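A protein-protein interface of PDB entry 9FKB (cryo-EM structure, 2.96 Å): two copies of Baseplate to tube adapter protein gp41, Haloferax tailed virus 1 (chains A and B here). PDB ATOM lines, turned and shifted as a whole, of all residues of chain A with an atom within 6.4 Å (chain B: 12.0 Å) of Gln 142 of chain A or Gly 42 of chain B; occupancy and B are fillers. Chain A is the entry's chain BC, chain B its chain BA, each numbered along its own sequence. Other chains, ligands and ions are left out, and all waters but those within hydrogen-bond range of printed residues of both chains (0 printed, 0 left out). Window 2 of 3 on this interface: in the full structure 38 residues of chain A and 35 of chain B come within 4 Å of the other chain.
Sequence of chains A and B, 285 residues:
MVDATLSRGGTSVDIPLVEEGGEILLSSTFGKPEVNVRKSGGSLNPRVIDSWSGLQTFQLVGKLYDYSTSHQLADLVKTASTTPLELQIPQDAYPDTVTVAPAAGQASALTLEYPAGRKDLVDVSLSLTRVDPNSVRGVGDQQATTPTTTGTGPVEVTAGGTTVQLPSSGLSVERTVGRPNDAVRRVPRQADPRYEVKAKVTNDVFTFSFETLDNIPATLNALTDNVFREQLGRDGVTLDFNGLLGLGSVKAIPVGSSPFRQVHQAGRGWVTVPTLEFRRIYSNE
O of Gly 42 of chain B lies within hydrogen-bond range of NE2 of Gln 142 of chain A (2.7 Å). O of Ala 199 of chain A sits close to O of Gly 41 of chain B, at 3.1 Å. The side-chain amide oxygen (OD1) of Asn 45 of chain B sits at hydrogen-bond distance from the side-chain amino group (NZ) of Lys 78 of chain A (2.8 Å).
N of Arg 38 of chain B is in hydrogen-bond range of O of Arg 47 of chain B, 3.1 Å away. The side-chain hydroxyl (OG1) of Thr 79 of chain A lies within hydrogen-bond range of the side-chain amide nitrogen (NE2) of Gln 143 of chain A, at 3.4 Å. The backbone NH of Ala 144 of chain A sits at hydrogen-bond distance from the side-chain hydroxyl of Thr 79 of chain A (2.9 Å). The backbone NH of Gln 142 of chain A is in hydrogen-bond range of the backbone carbonyl oxygen of Ala 80 of chain A. The backbone carbonyl oxygen of Lys 78 of chain A sits at hydrogen-bond distance from the guanidinium group of Arg 179 of chain A.
Ser 43 of chain B touches Gln 142 of chain A (CA to OE1, 3.3 Å). OE1 of Gln 142 of chain A touches N of Leu 44 of chain B, 3.7 Å away. O of Gln 143 of chain A touches CD1 of Leu 44 of chain B (3.5 Å). Ala 144 of chain A touches Leu 44 of chain B. Ala 199 of chain A touches Gly 42 of chain B. O of Gly 41 of chain B touches CA of Lys 200 of chain A, 3.6 Å away. O of Arg 38 of chain B touches CG2 of Val 201 of chain A, 3.8 Å away. Val 201 of chain A touches Ser 43 of chain B. O of Leu 44 of chain B touches CA of Val 201 of chain A (3.7 Å). CG2 of Val 201 of chain A touches CA of Pro 46 of chain B, 3.6 Å away.
Printed residues of chain B within 4 Å of Lys 78 of chain A: Asn 45. No residue of chain B comes within 4 Å of Ala 80 of chain A. No residue of chain B comes within 4 Å of Ser 81 of chain A. No residue of chain B comes within 4 Å of Gly 140 of chain A. No residue of chain B comes within 4 Å of Asp 141 of chain A. Gln 142 of chain A touches just these residues of chain B: Gly 42 (2.7 Å), Ser 43 (3.3 Å) and Leu 44 (3.7 Å). Ala 199 of chain A touches just these residues of chain B: Gly 41 and Gly 42. Of the printed residues of chain A, Gly 42 of chain B touches Gln 142 (2.7 Å) and Ala 199 (3.7 Å). Of the printed residues of chain A, Ser 43 of chain B touches Gln 142 and Val 201. Printed residues of chain A within 4 Å of Leu 44 of chain B: Gln 142 (3.7 Å), Gln 143 (3.5 Å), Ala 144 (3.4 Å) and Val 201 (3.7 Å). The nearest residue of chain B that does not touch Gln 142 of chain A is Gly 41 of chain B (5.8 Å). The nearest printed residue of chain B that does not touch Val 201 of chain A is Ser 40 of chain B (4.01 Å).
Among the printed residues, no Asp or Glu carboxylate lies within 4 Å of a Lys or Arg side-chain nitrogen of the other chain.
No position is printed for both chains.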
ATOM      1  N   LYS A  78     -15.459 -33.902  -1.941  1.00  0.00           N
ATOM      2  CA  LYS A  78     -14.303 -33.200  -2.473  1.00  0.00           C
ATOM      3  C   LYS A  78     -13.997 -31.915  -1.702  1.00  0.00           C
ATOM      4  O   LYS A  78     -12.839 -31.490  -1.674  1.00  0.00           O
ATOM      5  CB  LYS A  78     -14.484 -32.963  -3.970  1.00  0.00           C
ATOM      6  CG  LYS A  78     -13.182 -32.816  -4.732  1.00  0.00           C
ATOM      7  CD  LYS A  78     -13.334 -32.953  -6.239  1.00  0.00           C
ATOM      8  CE  LYS A  78     -13.885 -31.719  -6.932  1.00  0.00           C
ATOM      9  NZ  LYS A  78     -12.810 -30.798  -7.378  1.00  0.00           N
ATOM     10  N   THR A  79     -15.010 -31.311  -1.067  1.00  0.00           N
ATOM     11  CA  THR A  79     -14.908 -30.080  -0.282  1.00  0.00           C
ATOM     12  C   THR A  79     -13.788 -30.138   0.765  1.00  0.00           C
ATOM     13  O   THR A  79     -13.657 -31.119   1.488  1.00  0.00           O
ATOM     14  CB  THR A  79     -16.257 -29.775   0.393  1.00  0.00           C
ATOM     15  OG1 THR A  79     -17.135 -29.325  -0.628  1.00  0.00           O
ATOM     16  CG2 THR A  79     -16.240 -28.721   1.480  1.00  0.00           C
ATOM     17  N   ALA A  80     -13.003 -29.051   0.870  1.00  0.00           N
ATOM     18  CA  ALA A  80     -12.094 -28.831   1.988  1.00  0.00           C
ATOM     19  C   ALA A  80     -12.881 -28.165   3.120  1.00  0.00           C
ATOM     20  O   ALA A  80     -13.420 -27.079   2.929  1.00  0.00           O
ATOM     21  CB  ALA A  80     -10.942 -27.960   1.538  1.00  0.00           C
ATOM     22  N   SER A  81     -12.962 -28.812   4.298  1.00  0.00           N
ATOM     23  CA  SER A  81     -13.516 -28.158   5.478  1.00  0.00           C
ATOM     24  C   SER A  81     -12.861 -28.695   6.749  1.00  0.00           C
ATOM     25  O   SER A  81     -12.603 -29.888   6.844  1.00  0.00           O
ATOM     26  CB  SER A  81     -15.025 -28.293   5.527  1.00  0.00           C
ATOM     27  OG  SER A  81     -15.527 -27.668   6.699  1.00  0.00           O
ATOM     28  N   VAL A 139      -6.712 -25.969   6.742  1.00  0.00           N
ATOM     29  CA  VAL A 139      -6.405 -24.623   6.261  1.00  0.00           C
ATOM     30  C   VAL A 139      -7.638 -24.034   5.557  1.00  0.00           C
ATOM     31  O   VAL A 139      -7.836 -24.196   4.346  1.00  0.00           O
ATOM     32  CB  VAL A 139      -5.136 -24.607   5.377  1.00  0.00           C
ATOM     33  CG1 VAL A 139      -4.746 -23.192   4.956  1.00  0.00           C
ATOM     34  CG2 VAL A 139      -3.959 -25.296   6.053  1.00  0.00           C
ATOM     35  N   GLY A 140      -8.479 -23.343   6.347  1.00  0.00           N
ATOM     36  CA  GLY A 140      -9.726 -22.737   5.891  1.00  0.00           C
ATOM     37  C   GLY A 140     -10.780 -23.742   5.403  1.00  0.00           C
ATOM     38  O   GLY A 140     -10.672 -24.955   5.608  1.00  0.00           O
ATOM     39  N   ASP A 141     -11.821 -23.207   4.745  1.00  0.00           N
ATOM     40  CA  ASP A 141     -12.873 -23.979   4.083  1.00  0.00           C
ATOM     41  C   ASP A 141     -12.992 -23.569   2.609  1.00  0.00           C
ATOM     42  O   ASP A 141     -12.924 -22.384   2.275  1.00  0.00           O
ATOM     43  CB  ASP A 141     -14.228 -23.854   4.801  1.00  0.00           C
ATOM     44  CG  ASP A 141     -14.216 -24.156   6.296  1.00  0.00           C
ATOM     45  OD1 ASP A 141     -14.361 -25.340   6.678  1.00  0.00           O
ATOM     46  OD2 ASP A 141     -14.099 -23.185   7.085  1.00  0.00           O
ATOM     47  N   GLN A 142     -13.175 -24.562   1.719  1.00  0.00           N
ATOM     48  CA  GLN A 142     -13.397 -24.368   0.288  1.00  0.00           C
ATOM     49  C   GLN A 142     -14.426 -25.385  -0.219  1.00  0.00           C
ATOM     50  O   GLN A 142     -14.124 -26.569  -0.368  1.00  0.00           O
ATOM     51  CB  GLN A 142     -12.083 -24.466  -0.489  1.00  0.00           C
ATOM     52  CG  GLN A 142     -11.049 -23.395  -0.138  1.00  0.00           C
ATOM     53  CD  GLN A 142      -9.940 -23.208  -1.146  1.00  0.00           C
ATOM     54  OE1 GLN A 142      -9.677 -24.069  -1.983  1.00  0.00           O
ATOM     55  NE2 GLN A 142      -9.258 -22.072  -1.060  1.00  0.00           N
ATOM     56  N   GLN A 143     -15.649 -24.901  -0.481  1.00  0.00           N
ATOM     57  CA  GLN A 143     -16.772 -25.703  -0.962  1.00  0.00           C
ATOM     58  C   GLN A 143     -16.541 -26.099  -2.428  1.00  0.00           C
ATOM     59  O   GLN A 143     -16.406 -25.234  -3.299  1.00  0.00           O
ATOM     60  CB  GLN A 143     -18.065 -24.896  -0.764  1.00  0.00           C
ATOM     61  CG  GLN A 143     -19.327 -25.548  -1.333  1.00  0.00           C
ATOM     62  CD  GLN A 143     -19.759 -26.795  -0.597  1.00  0.00           C
ATOM     63  OE1 GLN A 143     -19.785 -26.823   0.633  1.00  0.00           O
ATOM     64  NE2 GLN A 143     -20.117 -27.837  -1.335  1.00  0.00           N
ATOM     65  N   ALA A 144     -16.535 -27.414  -2.712  1.00  0.00           N
ATOM     66  CA  ALA A 144     -16.553 -27.917  -4.082  1.00  0.00           C
ATOM     67  C   ALA A 144     -17.922 -27.665  -4.727  1.00  0.00           C
ATOM     68  O   ALA A 144     -18.968 -27.745  -4.062  1.00  0.00           O
ATOM     69  CB  ALA A 144     -16.186 -29.381  -4.100  1.00  0.00           C
ATOM     70  N   ARG A 179      -9.208 -36.883  -2.631  1.00  0.00           N
ATOM     71  CA  ARG A 179      -8.401 -35.893  -1.928  1.00  0.00           C
ATOM     72  C   ARG A 179      -7.001 -36.452  -1.655  1.00  0.00           C
ATOM     73  O   ARG A 179      -6.595 -36.608  -0.505  1.00  0.00           O
ATOM     74  CB  ARG A 179      -9.138 -35.390  -0.681  1.00  0.00           C
ATOM     75  CG  ARG A 179     -10.358 -34.524  -0.979  1.00  0.00           C
ATOM     76  CD  ARG A 179     -10.880 -33.765   0.231  1.00  0.00           C
ATOM     77  NE  ARG A 179      -9.825 -32.908   0.758  1.00  0.00           N
ATOM     78  CZ  ARG A 179      -9.565 -31.639   0.443  1.00  0.00           C
ATOM     79  NH1 ARG A 179      -8.530 -31.037   0.987  1.00  0.00           N
ATOM     80  NH2 ARG A 179     -10.300 -30.961  -0.411  1.00  0.00           N
ATOM     81  N   ALA A 199      -4.357 -27.235   2.011  1.00  0.00           N
ATOM     82  CA  ALA A 199      -4.569 -26.263   0.945  1.00  0.00           C
ATOM     83  C   ALA A 199      -3.828 -26.729  -0.319  1.00  0.00           C
ATOM     84  O   ALA A 199      -2.845 -26.124  -0.769  1.00  0.00           O
ATOM     85  CB  ALA A 199      -4.182 -24.871   1.415  1.00  0.00           C
ATOM     86  N   LYS A 200      -4.318 -27.853  -0.878  1.00  0.00           N
ATOM     87  CA  LYS A 200      -3.758 -28.489  -2.065  1.00  0.00           C
ATOM     88  C   LYS A 200      -4.860 -28.988  -3.002  1.00  0.00           C
ATOM     89  O   LYS A 200      -5.997 -29.236  -2.598  1.00  0.00           O
ATOM     90  CB  LYS A 200      -2.782 -29.602  -1.676  1.00  0.00           C
ATOM     91  CG  LYS A 200      -1.434 -29.113  -1.165  1.00  0.00           C
ATOM     92  CD  LYS A 200      -0.503 -30.264  -0.843  1.00  0.00           C
ATOM     93  CE  LYS A 200       0.890 -29.801  -0.463  1.00  0.00           C
ATOM     94  NZ  LYS A 200       1.827 -30.939  -0.304  1.00  0.00           N
ATOM     95  N   VAL A 201      -4.460 -29.161  -4.266  1.00  0.00           N
ATOM     96  CA  VAL A 201      -5.296 -29.582  -5.383  1.00  0.00           C
ATOM     97  C   VAL A 201      -5.964 -30.944  -5.126  1.00  0.00           C
ATOM     98  O   VAL A 201      -5.359 -31.880  -4.595  1.00  0.00           O
ATOM     99  CB  VAL A 201      -4.452 -29.541  -6.675  1.00  0.00           C
ATOM    100  CG1 VAL A 201      -4.955 -30.474  -7.771  1.00  0.00           C
ATOM    101  CG2 VAL A 201      -4.274 -28.119  -7.186  1.00  0.00           C
ATOM    102  N   ARG B  38      -0.301 -28.298 -11.773  1.00  0.00           N
ATOM    103  CA  ARG B  38       0.058 -27.821 -10.443  1.00  0.00           C
ATOM    104  C   ARG B  38      -0.336 -28.856  -9.382  1.00  0.00           C
ATOM    105  O   ARG B  38      -1.464 -29.330  -9.376  1.00  0.00           O
ATOM    106  CB  ARG B  38      -0.633 -26.482 -10.148  1.00  0.00           C
ATOM    107  CG  ARG B  38      -0.168 -25.295 -10.984  1.00  0.00           C
ATOM    108  CD  ARG B  38       1.318 -24.989 -11.038  1.00  0.00           C
ATOM    109  NE  ARG B  38       1.559 -23.610 -11.470  1.00  0.00           N
ATOM    110  CZ  ARG B  38       2.751 -23.065 -11.713  1.00  0.00           C
ATOM    111  NH1 ARG B  38       2.823 -21.801 -12.099  1.00  0.00           N
ATOM    112  NH2 ARG B  38       3.858 -23.778 -11.575  1.00  0.00           N
ATOM    113  N   LYS B  39       0.570 -29.135  -8.424  1.00  0.00           N
ATOM    114  CA  LYS B  39       0.323 -30.045  -7.301  1.00  0.00           C
ATOM    115  C   LYS B  39      -0.162 -29.328  -6.030  1.00  0.00           C
ATOM    116  O   LYS B  39      -0.525 -29.978  -5.044  1.00  0.00           O
ATOM    117  CB  LYS B  39       1.599 -30.830  -6.968  1.00  0.00           C
ATOM    118  CG  LYS B  39       2.183 -31.661  -8.105  1.00  0.00           C
ATOM    119  CD  LYS B  39       3.548 -32.260  -7.760  1.00  0.00           C
ATOM    120  CE  LYS B  39       3.536 -33.288  -6.639  1.00  0.00           C
ATOM    121  NZ  LYS B  39       4.894 -33.573  -6.108  1.00  0.00           N
ATOM    122  N   SER B  40      -0.172 -27.985  -6.040  1.00  0.00           N
ATOM    123  CA  SER B  40      -0.233 -27.166  -4.834  1.00  0.00           C
ATOM    124  C   SER B  40      -1.064 -25.892  -5.040  1.00  0.00           C
ATOM    125  O   SER B  40      -1.406 -25.515  -6.156  1.00  0.00           O
ATOM    126  CB  SER B  40       1.175 -26.845  -4.392  1.00  0.00           C
ATOM    127  OG  SER B  40       1.213 -26.270  -3.093  1.00  0.00           O
ATOM    128  N   GLY B  41      -1.403 -25.226  -3.929  1.00  0.00           N
ATOM    129  CA  GLY B  41      -2.198 -24.006  -3.935  1.00  0.00           C
ATOM    130  C   GLY B  41      -3.569 -24.201  -3.287  1.00  0.00           C
ATOM    131  O   GLY B  41      -4.204 -25.240  -3.464  1.00  0.00           O
ATOM    132  N   GLY B  42      -4.053 -23.164  -2.584  1.00  0.00           N
ATOM    133  CA  GLY B  42      -5.363 -23.165  -1.941  1.00  0.00           C
ATOM    134  C   GLY B  42      -6.508 -22.907  -2.925  1.00  0.00           C
ATOM    135  O   GLY B  42      -7.201 -21.890  -2.845  1.00  0.00           O
ATOM    136  N   SER B  43      -6.683 -23.828  -3.883  1.00  0.00           N
ATOM    137  CA  SER B  43      -7.836 -23.918  -4.770  1.00  0.00           C
ATOM    138  C   SER B  43      -8.077 -25.388  -5.102  1.00  0.00           C
ATOM    139  O   SER B  43      -7.133 -26.168  -5.228  1.00  0.00           O
ATOM    140  CB  SER B  43      -7.651 -23.088  -6.013  1.00  0.00           C
ATOM    141  OG  SER B  43      -7.661 -21.705  -5.689  1.00  0.00           O
ATOM    142  N   LEU B  44      -9.352 -25.774  -5.271  1.00  0.00           N
ATOM    143  CA  LEU B  44      -9.703 -27.191  -5.339  1.00  0.00           C
ATOM    144  C   LEU B  44      -9.211 -27.842  -6.633  1.00  0.00           C
ATOM    145  O   LEU B  44      -8.749 -28.988  -6.620  1.00  0.00           O
ATOM    146  CB  LEU B  44     -11.217 -27.355  -5.201  1.00  0.00           C
ATOM    147  CG  LEU B  44     -11.821 -26.846  -3.895  1.00  0.00           C
ATOM    148  CD1 LEU B  44     -13.327 -26.789  -4.011  1.00  0.00           C
ATOM    149  CD2 LEU B  44     -11.394 -27.698  -2.706  1.00  0.00           C
ATOM    150  N   ASN B  45      -9.341 -27.108  -7.746  1.00  0.00           N
ATOM    151  CA  ASN B  45      -9.028 -27.605  -9.077  1.00  0.00           C
ATOM    152  C   ASN B  45      -7.679 -27.045  -9.531  1.00  0.00           C
ATOM    153  O   ASN B  45      -7.408 -25.865  -9.345  1.00  0.00           O
ATOM    154  CB  ASN B  45     -10.174 -27.278 -10.041  1.00  0.00           C
ATOM    155  CG  ASN B  45     -11.547 -27.684  -9.534  1.00  0.00           C
ATOM    156  OD1 ASN B  45     -11.729 -28.791  -9.034  1.00  0.00           O
ATOM    157  ND2 ASN B  45     -12.532 -26.806  -9.680  1.00  0.00           N
ATOM    158  N   PRO B  46      -6.797 -27.859 -10.153  1.00  0.00           N
ATOM    159  CA  PRO B  46      -5.461 -27.398 -10.531  1.00  0.00           C
ATOM    160  C   PRO B  46      -5.450 -26.423 -11.704  1.00  0.00           C
ATOM    161  O   PRO B  46      -6.132 -26.641 -12.708  1.00  0.00           O
ATOM    162  CB  PRO B  46      -4.745 -28.684 -10.969  1.00  0.00           C
ATOM    163  CG  PRO B  46      -5.846 -29.648 -11.356  1.00  0.00           C
ATOM    164  CD  PRO B  46      -7.046 -29.259 -10.523  1.00  0.00           C
ATOM    165  N   ARG B  47      -4.618 -25.375 -11.591  1.00  0.00           N
ATOM    166  CA  ARG B  47      -4.141 -24.653 -12.767  1.00  0.00           C
ATOM    167  C   ARG B  47      -3.150 -25.542 -13.533  1.00  0.00           C
ATOM    168  O   ARG B  47      -2.508 -26.423 -12.946  1.00  0.00           O
ATOM    169  CB  ARG B  47      -3.512 -23.296 -12.409  1.00  0.00           C
ATOM    170  CG  ARG B  47      -4.371 -22.368 -11.559  1.00  0.00           C
ATOM    171  CD  ARG B  47      -3.635 -21.259 -10.811  1.00  0.00           C
ATOM    172  NE  ARG B  47      -4.500 -20.614  -9.815  1.00  0.00           N
ATOM    173  CZ  ARG B  47      -4.922 -19.345  -9.832  1.00  0.00           C
ATOM    174  NH1 ARG B  47      -5.712 -18.900  -8.865  1.00  0.00           N
ATOM    175  NH2 ARG B  47      -4.545 -18.516 -10.793  1.00  0.00           N
